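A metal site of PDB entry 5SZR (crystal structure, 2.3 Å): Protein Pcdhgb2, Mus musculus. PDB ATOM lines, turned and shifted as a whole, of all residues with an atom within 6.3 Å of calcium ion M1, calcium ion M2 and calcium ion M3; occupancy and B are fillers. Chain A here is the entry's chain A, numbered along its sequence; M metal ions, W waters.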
ATOM      1  N   GLU A 226       7.530   1.108  32.084  1.00  0.00           N
ATOM      2  CA  GLU A 226       8.005  -0.052  32.810  1.00  0.00           C
ATOM      3  C   GLU A 226       9.417   0.151  33.336  1.00  0.00           C
ATOM      4  O   GLU A 226      10.182   0.955  32.807  1.00  0.00           O
ATOM      5  CB  GLU A 226       7.952  -1.259  31.863  1.00  0.00           C
ATOM      6  CG  GLU A 226       8.407  -2.576  32.370  1.00  0.00           C
ATOM      7  CD  GLU A 226       8.175  -3.654  31.341  1.00  0.00           C
ATOM      8  OE1 GLU A 226       8.494  -3.416  30.154  1.00  0.00           O
ATOM      9  OE2 GLU A 226       7.641  -4.714  31.704  1.00  0.00           O
ATOM     10  N   ASN A 227       9.748  -0.587  34.400  1.00  0.00           N
ATOM     11  CA  ASN A 227      11.080  -0.640  34.988  1.00  0.00           C
ATOM     12  C   ASN A 227      11.502   0.685  35.606  1.00  0.00           C
ATOM     13  O   ASN A 227      12.688   0.946  35.806  1.00  0.00           O
ATOM     14  CB  ASN A 227      12.122  -1.109  33.965  1.00  0.00           C
ATOM     15  CG  ASN A 227      11.781  -2.462  33.375  1.00  0.00           C
ATOM     16  OD1 ASN A 227      11.265  -3.338  34.071  1.00  0.00           O
ATOM     17  ND2 ASN A 227      12.045  -2.636  32.088  1.00  0.00           N
ATOM     18  N   PHE A 283       7.409  -1.170  37.990  1.00  0.00           N
ATOM     19  CA  PHE A 283       6.343  -1.840  37.272  1.00  0.00           C
ATOM     20  C   PHE A 283       6.915  -2.757  36.183  1.00  0.00           C
ATOM     21  O   PHE A 283       7.954  -2.469  35.592  1.00  0.00           O
ATOM     22  CB  PHE A 283       5.383  -0.821  36.655  1.00  0.00           C
ATOM     23  CG  PHE A 283       4.674   0.027  37.671  1.00  0.00           C
ATOM     24  CD1 PHE A 283       4.343   1.345  37.393  1.00  0.00           C
ATOM     25  CD2 PHE A 283       4.315  -0.488  38.912  1.00  0.00           C
ATOM     26  CE1 PHE A 283       3.687   2.142  38.328  1.00  0.00           C
ATOM     27  CE2 PHE A 283       3.652   0.303  39.851  1.00  0.00           C
ATOM     28  CZ  PHE A 283       3.334   1.610  39.555  1.00  0.00           C
ATOM     29  N   ASP A 284       6.212  -3.855  35.926  1.00  0.00           N
ATOM     30  CA  ASP A 284       6.600  -4.841  34.912  1.00  0.00           C
ATOM     31  C   ASP A 284       5.410  -5.023  33.979  1.00  0.00           C
ATOM     32  O   ASP A 284       4.413  -5.649  34.349  1.00  0.00           O
ATOM     33  CB  ASP A 284       7.013  -6.157  35.575  1.00  0.00           C
ATOM     34  CG  ASP A 284       7.360  -7.244  34.564  1.00  0.00           C
ATOM     35  OD1 ASP A 284       7.586  -6.943  33.378  1.00  0.00           O
ATOM     36  OD2 ASP A 284       7.444  -8.421  34.986  1.00  0.00           O
ATOM     37  N   HIS A 285       5.522  -4.459  32.773  1.00  0.00           N
ATOM     38  CA  HIS A 285       4.411  -4.496  31.815  1.00  0.00           C
ATOM     39  C   HIS A 285       3.977  -5.921  31.512  1.00  0.00           C
ATOM     40  O   HIS A 285       2.803  -6.168  31.203  1.00  0.00           O
ATOM     41  CB  HIS A 285       4.817  -3.778  30.530  1.00  0.00           C
ATOM     42  CG  HIS A 285       3.830  -3.921  29.412  1.00  0.00           C
ATOM     43  ND1 HIS A 285       2.768  -3.063  29.237  1.00  0.00           N
ATOM     44  CD2 HIS A 285       3.755  -4.830  28.408  1.00  0.00           C
ATOM     45  CE1 HIS A 285       2.069  -3.438  28.171  1.00  0.00           C
ATOM     46  NE2 HIS A 285       2.651  -4.503  27.646  1.00  0.00           N
ATOM     47  N   GLU A 286       4.895  -6.885  31.597  1.00  0.00           N
ATOM     48  CA  GLU A 286       4.561  -8.267  31.286  1.00  0.00           C
ATOM     49  C   GLU A 286       3.704  -8.918  32.384  1.00  0.00           C
ATOM     50  O   GLU A 286       3.003  -9.892  32.087  1.00  0.00           O
ATOM     51  CB  GLU A 286       5.833  -9.067  31.059  1.00  0.00           C
ATOM     52  CG  GLU A 286       6.438  -8.882  29.648  1.00  0.00           C
ATOM     53  CD  GLU A 286       6.999  -7.483  29.403  1.00  0.00           C
ATOM     54  OE1 GLU A 286       7.763  -6.983  30.238  1.00  0.00           O
ATOM     55  OE2 GLU A 286       6.667  -6.886  28.357  1.00  0.00           O
ATOM     56  N   GLN A 287       3.737  -8.396  33.606  1.00  0.00           N
ATOM     57  CA  GLN A 287       2.871  -8.906  34.669  1.00  0.00           C
ATOM     58  C   GLN A 287       1.537  -8.160  34.728  1.00  0.00           C
ATOM     59  O   GLN A 287       0.480  -8.785  34.836  1.00  0.00           O
ATOM     60  CB  GLN A 287       3.579  -8.831  36.023  1.00  0.00           C
ATOM     61  CG  GLN A 287       4.680  -9.873  36.198  1.00  0.00           C
ATOM     62  CD  GLN A 287       4.180 -11.293  36.063  1.00  0.00           C
ATOM     63  OE1 GLN A 287       3.148 -11.656  36.632  1.00  0.00           O
ATOM     64  NE2 GLN A 287       4.893 -12.100  35.291  1.00  0.00           N
ATOM     65  N   GLY A 316       3.657   1.203  30.685  1.00  0.00           N
ATOM     66  CA  GLY A 316       4.144   1.235  29.319  1.00  0.00           C
ATOM     67  C   GLY A 316       5.140   0.122  29.044  1.00  0.00           C
ATOM     68  O   GLY A 316       5.975  -0.205  29.877  1.00  0.00           O
ATOM     69  N   ASP A 317       5.038  -0.454  27.848  1.00  0.00           N
ATOM     70  CA  ASP A 317       5.915  -1.536  27.453  1.00  0.00           C
ATOM     71  C   ASP A 317       7.266  -1.000  27.006  1.00  0.00           C
ATOM     72  O   ASP A 317       7.337  -0.072  26.189  1.00  0.00           O
ATOM     73  CB  ASP A 317       5.274  -2.363  26.332  1.00  0.00           C
ATOM     74  CG  ASP A 317       6.124  -3.544  25.921  1.00  0.00           C
ATOM     75  OD1 ASP A 317       6.793  -4.130  26.805  1.00  0.00           O
ATOM     76  OD2 ASP A 317       6.112  -3.901  24.727  1.00  0.00           O
ATOM     77  N   ARG A 318       8.337  -1.555  27.547  1.00  0.00           N
ATOM     78  CA  ARG A 318       9.688  -1.339  27.057  1.00  0.00           C
ATOM     79  C   ARG A 318      10.242  -2.623  26.465  1.00  0.00           C
ATOM     80  O   ARG A 318       9.702  -3.719  26.687  1.00  0.00           O
ATOM     81  CB  ARG A 318      10.621  -0.837  28.177  1.00  0.00           C
ATOM     82  CG  ARG A 318      10.463   0.628  28.535  1.00  0.00           C
ATOM     83  CD  ARG A 318      11.593   1.074  29.444  1.00  0.00           C
ATOM     84  NE  ARG A 318      11.499   2.481  29.805  1.00  0.00           N
ATOM     85  CZ  ARG A 318      11.924   3.481  29.027  1.00  0.00           C
ATOM     86  NH1 ARG A 318      11.800   4.732  29.434  1.00  0.00           N
ATOM     87  NH2 ARG A 318      12.466   3.211  27.848  1.00  0.00           N
ATOM     88  N   ASN A 319      11.323  -2.494  25.712  1.00  0.00           N
ATOM     89  CA  ASN A 319      11.958  -3.650  25.073  1.00  0.00           C
ATOM     90  C   ASN A 319      13.014  -4.232  26.006  1.00  0.00           C
ATOM     91  O   ASN A 319      14.220  -4.163  25.777  1.00  0.00           O
ATOM     92  CB  ASN A 319      12.561  -3.251  23.723  1.00  0.00           C
ATOM     93  CG  ASN A 319      12.951  -4.466  22.908  1.00  0.00           C
ATOM     94  OD1 ASN A 319      12.258  -5.478  22.924  1.00  0.00           O
ATOM     95  ND2 ASN A 319      14.084  -4.389  22.198  1.00  0.00           N
ATOM     96  N   ASP A 320      12.527  -4.847  27.092  1.00  0.00           N
ATOM     97  CA  ASP A 320      13.406  -5.480  28.061  1.00  0.00           C
ATOM     98  C   ASP A 320      13.455  -6.994  27.919  1.00  0.00           C
ATOM     99  O   ASP A 320      13.952  -7.686  28.817  1.00  0.00           O
ATOM    100  CB  ASP A 320      13.007  -5.080  29.488  1.00  0.00           C
ATOM    101  CG  ASP A 320      11.527  -5.308  29.775  1.00  0.00           C
ATOM    102  OD1 ASP A 320      10.752  -5.524  28.832  1.00  0.00           O
ATOM    103  OD2 ASP A 320      11.147  -5.244  30.969  1.00  0.00           O
ATOM    104  N   ASN A 321      12.961  -7.544  26.811  1.00  0.00           N
ATOM    105  CA  ASN A 321      13.047  -8.970  26.534  1.00  0.00           C
ATOM    106  C   ASN A 321      13.591  -9.157  25.125  1.00  0.00           C
ATOM    107  O   ASN A 321      13.046  -8.616  24.168  1.00  0.00           O
ATOM    108  CB  ASN A 321      11.685  -9.653  26.666  1.00  0.00           C
ATOM    109  CG  ASN A 321      11.204  -9.701  28.097  1.00  0.00           C
ATOM    110  OD1 ASN A 321      11.515 -10.637  28.831  1.00  0.00           O
ATOM    111  ND2 ASN A 321      10.436  -8.696  28.496  1.00  0.00           N
ATOM    112  N   ALA A 322      14.680  -9.914  25.012  1.00  0.00           N
ATOM    113  CA  ALA A 322      15.205 -10.281  23.711  1.00  0.00           C
ATOM    114  C   ALA A 322      14.438 -11.468  23.153  1.00  0.00           C
ATOM    115  O   ALA A 322      13.999 -12.339  23.921  1.00  0.00           O
ATOM    116  CB  ALA A 322      16.688 -10.616  23.794  1.00  0.00           C
ATOM    117  N   PRO A 323      14.248 -11.536  21.836  1.00  0.00           N
ATOM    118  CA  PRO A 323      13.629 -12.730  21.258  1.00  0.00           C
ATOM    119  C   PRO A 323      14.469 -13.963  21.541  1.00  0.00           C
ATOM    120  O   PRO A 323      15.684 -13.895  21.712  1.00  0.00           O
ATOM    121  CB  PRO A 323      13.570 -12.411  19.756  1.00  0.00           C
ATOM    122  CG  PRO A 323      14.507 -11.280  19.542  1.00  0.00           C
ATOM    123  CD  PRO A 323      14.570 -10.511  20.828  1.00  0.00           C
ATOM    124  N   ASP A 358       8.759 -13.633  21.696  1.00  0.00           N
ATOM    125  CA  ASP A 358       9.236 -12.413  22.334  1.00  0.00           C
ATOM    126  C   ASP A 358       8.218 -12.001  23.393  1.00  0.00           C
ATOM    127  O   ASP A 358       7.039 -11.831  23.081  1.00  0.00           O
ATOM    128  CB  ASP A 358       9.426 -11.295  21.301  1.00  0.00           C
ATOM    129  CG  ASP A 358      10.287 -10.160  21.824  1.00  0.00           C
ATOM    130  OD1 ASP A 358       9.945  -9.558  22.864  1.00  0.00           O
ATOM    131  OD2 ASP A 358      11.312  -9.854  21.183  1.00  0.00           O
ATOM    132  N   ALA A 359       8.676 -11.847  24.636  1.00  0.00           N
ATOM    133  CA  ALA A 359       7.782 -11.595  25.761  1.00  0.00           C
ATOM    134  C   ALA A 359       7.161 -10.210  25.742  1.00  0.00           C
ATOM    135  O   ALA A 359       6.222  -9.955  26.507  1.00  0.00           O
ATOM    136  CB  ALA A 359       8.515 -11.812  27.081  1.00  0.00           C
ATOM    137  N   ASP A 360       7.655  -9.296  24.909  1.00  0.00           N
ATOM    138  CA  ASP A 360       7.179  -7.919  24.940  1.00  0.00           C
ATOM    139  C   ASP A 360       5.891  -7.759  24.133  1.00  0.00           C
ATOM    140  O   ASP A 360       5.232  -8.762  23.816  1.00  0.00           O
ATOM    141  CB  ASP A 360       8.270  -6.977  24.418  1.00  0.00           C
ATOM    142  CG  ASP A 360       9.511  -7.001  25.289  1.00  0.00           C
ATOM    143  OD1 ASP A 360       9.371  -7.100  26.524  1.00  0.00           O
ATOM    144  OD2 ASP A 360      10.630  -6.911  24.755  1.00  0.00           O
ATOM    145  N   SER A 361       5.530  -6.521  23.806  1.00  0.00           N
ATOM    146  CA  SER A 361       4.311  -6.227  23.071  1.00  0.00           C
ATOM    147  C   SER A 361       4.601  -5.247  21.936  1.00  0.00           C
ATOM    148  O   SER A 361       5.665  -4.615  21.902  1.00  0.00           O
ATOM    149  CB  SER A 361       3.221  -5.648  23.990  1.00  0.00           C
ATOM    150  OG  SER A 361       2.947  -6.537  25.057  1.00  0.00           O
ATOM    151  N   HIS A 363       5.660  -3.282  18.710  1.00  0.00           N
ATOM    152  CA  HIS A 363       6.890  -3.368  17.935  1.00  0.00           C
ATOM    153  C   HIS A 363       8.014  -4.011  18.722  1.00  0.00           C
ATOM    154  O   HIS A 363       8.923  -4.609  18.133  1.00  0.00           O
ATOM    155  CB  HIS A 363       7.311  -1.977  17.447  1.00  0.00           C
ATOM    156  CG  HIS A 363       6.479  -1.469  16.301  1.00  0.00           C
ATOM    157  ND1 HIS A 363       5.264  -0.862  16.473  1.00  0.00           N
ATOM    158  CD2 HIS A 363       6.714  -1.487  14.966  1.00  0.00           C
ATOM    159  CE1 HIS A 363       4.771  -0.517  15.295  1.00  0.00           C
ATOM    160  NE2 HIS A 363       5.628  -0.887  14.363  1.00  0.00           N
ATOM    161  N   ASN A 364       7.983  -3.906  20.050  1.00  0.00           N
ATOM    162  CA  ASN A 364       9.016  -4.540  20.862  1.00  0.00           C
ATOM    163  C   ASN A 364       9.012  -6.062  20.713  1.00  0.00           C
ATOM    164  O   ASN A 364      10.010  -6.715  21.048  1.00  0.00           O
ATOM    165  CB  ASN A 364       8.847  -4.165  22.340  1.00  0.00           C
ATOM    166  CG  ASN A 364       9.139  -2.697  22.602  1.00  0.00           C
ATOM    167  OD1 ASN A 364      10.050  -2.117  22.031  1.00  0.00           O
ATOM    168  ND2 ASN A 364       8.359  -2.096  23.507  1.00  0.00           N
ATOM    169  N   ALA A 365       7.922  -6.644  20.184  1.00  0.00           N
ATOM    170  CA  ALA A 365       7.860  -8.087  19.972  1.00  0.00           C
ATOM    171  C   ALA A 365       7.503  -8.448  18.527  1.00  0.00           C
ATOM    172  O   ALA A 365       7.108  -9.587  18.260  1.00  0.00           O
ATOM    173  CB  ALA A 365       6.853  -8.733  20.932  1.00  0.00           C
ATOM    174  N   LEU A 367       8.697  -9.623  15.272  1.00  0.00           N
ATOM    175  CA  LEU A 367       9.937 -10.277  14.898  1.00  0.00           C
ATOM    176  C   LEU A 367      10.151 -10.246  13.391  1.00  0.00           C
ATOM    177  O   LEU A 367       9.207 -10.337  12.608  1.00  0.00           O
ATOM    178  CB  LEU A 367       9.948 -11.723  15.401  1.00  0.00           C
ATOM    179  CG  LEU A 367       9.747 -11.784  16.914  1.00  0.00           C
ATOM    180  CD1 LEU A 367      10.033 -13.178  17.432  1.00  0.00           C
ATOM    181  CD2 LEU A 367      10.607 -10.729  17.621  1.00  0.00           C
ATOM    182  N   ASP A 411      13.704  -8.060  16.987  1.00  0.00           N
ATOM    183  CA  ASP A 411      12.441  -7.401  17.249  1.00  0.00           C
ATOM    184  C   ASP A 411      12.453  -6.014  16.623  1.00  0.00           C
ATOM    185  O   ASP A 411      13.435  -5.585  16.010  1.00  0.00           O
ATOM    186  CB  ASP A 411      12.117  -7.376  18.742  1.00  0.00           C
ATOM    187  CG  ASP A 411      13.167  -6.641  19.579  1.00  0.00           C
ATOM    188  OD1 ASP A 411      13.826  -5.705  19.077  1.00  0.00           O
ATOM    189  OD2 ASP A 411      13.323  -6.999  20.762  1.00  0.00           O
ATOM    190  N   GLY A 412      11.350  -5.288  16.767  1.00  0.00           N
ATOM    191  CA  GLY A 412      11.234  -3.977  16.153  1.00  0.00           C
ATOM    192  C   GLY A 412      11.479  -2.849  17.128  1.00  0.00           C
ATOM    193  O   GLY A 412      11.117  -1.699  16.851  1.00  0.00           O
ATOM    194  N   GLY A 413      12.088  -3.156  18.268  1.00  0.00           N
ATOM    195  CA  GLY A 413      12.385  -2.162  19.267  1.00  0.00           C
ATOM    196  C   GLY A 413      13.554  -1.272  18.888  1.00  0.00           C
ATOM    197  O   GLY A 413      14.213  -1.448  17.858  1.00  0.00           O
ATOM    198  N   LEU A 417      16.760  -5.775  19.979  1.00  0.00           N
ATOM    199  CA  LEU A 417      17.363  -6.992  20.518  1.00  0.00           C
ATOM    200  C   LEU A 417      17.175  -8.143  19.537  1.00  0.00           C
ATOM    201  O   LEU A 417      16.240  -8.145  18.724  1.00  0.00           O
ATOM    202  CB  LEU A 417      16.740  -7.345  21.877  1.00  0.00           C
ATOM    203  CG  LEU A 417      16.771  -6.264  22.953  1.00  0.00           C
ATOM    204  CD1 LEU A 417      16.031  -6.722  24.197  1.00  0.00           C
ATOM    205  CD2 LEU A 417      18.207  -5.883  23.301  1.00  0.00           C
HETATM  206 CA    CA M   1      11.531  -7.615  22.587  1.00  0.00          CA
HETATM  207 CA    CA M   2       8.469  -5.376  28.110  1.00  0.00          CA
HETATM  208 CA    CA M   3       9.282  -6.318  31.849  1.00  0.00          CA
HETATM  209  O   HOH W   1      10.208  -5.832  34.008  1.00  0.00           O
HETATM  210  O   HOH W   2      10.345  -8.671  31.669  1.00  0.00           O
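The backbone NH of Glu 226 lies close to the backbone carbonyl oxygen of Gly 316 (3.0 Å). The side-chain carboxylate (OD1) of Asp 320 sits close to the side-chain amide nitrogen (ND2) of Asn 321 (3.2 Å). The side-chain amide nitrogen of Asn 227 lies close to the side-chain carboxylate of Asp 320. OD2 of Asp 317 lies within hydrogen-bond range of ND2 of Asn 364 (3.1 Å). The side-chain carboxylate (OD2) of Asp 317 sits at hydrogen-bond distance from the backbone NH (N) of Ser 361, at 2.8 Å. OD1 of Asp 411 sits at hydrogen-bond distance from N of Leu 417 (3.1 Å). OD1 of Asp 411 lies within hydrogen-bond range of N of Gly 413 (3.2 Å).
Six residues have an atom within 4 Å of calcium ion M1: Asn 319, Asn 321, Asp 358, Asp 360, Asn 364 and Asp 411. The nearest printed residue that does not touch calcium ion M1 is Ala 365 (4.4 Å).
Of the 27 residues printed, 4 come within 4 Å of calcium ion M3. Along chain A the residues within 4 Å of calcium ion M3 span positions 226 to 320. The nearest printed residue that does not touch calcium ion M3 is Asn 227 (4.2 Å).
OD1 of Asn 319 is bound to calcium ion M1 (2.3 Å). Calcium ion M1 is bound by O of Asn 364, 2.3 Å away. The backbone carbonyl oxygen (O) of Asn 321 binds calcium ion M1. Calcium ion M1 is bound by the side-chain carboxylate (OD2) of Asp 360. Calcium ion M1 is bound by the side-chain carboxylate (OD1) of Asp 358 (2.5 Å). Calcium ion M1 is bound by the side-chain carboxylate (OD2) of Asp 411, 2.6 Å away. OD2 of Asp 358 is bound to calcium ion M1, at 2.7 Å. Calcium ion M1 has seven donor atoms within binding distance.
Calcium ion M2 is bound by the side-chain carboxylate (OE2) of Glu 286, 2.4 Å away. OD1 of Asp 320 binds calcium ion M2 (2.4 Å). The side-chain carboxylate (OD1) of Asp 317 is bound to calcium ion M2 (2.5 Å). Calcium ion M2 is bound by the backbone carbonyl oxygen (O) of Arg 318 (2.5 Å). Calcium ion M2 is bound by OD1 of Asp 360. OE1 of Glu 286 binds calcium ion M2 (2.8 Å). Calcium ion M2 is bound by OE1 of Glu 226, at 2.8 Å.
OE2 of Glu 226 is bound to calcium ion M3 (2.3 Å). Calcium ion M3 is bound by OE1 of Glu 286. OD2 of Asp 320 is bound to calcium ion M3 (2.3 Å). Calcium ion M3 is bound by the side-chain carboxylate (OD1) of Asp 284, 2.4 Å away. Calcium ion M3 is bound by water W1 (2.4 Å). Water W2 is bound to calcium ion M3 (2.6 Å). Calcium ion M3 has six donor atoms within binding distance.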
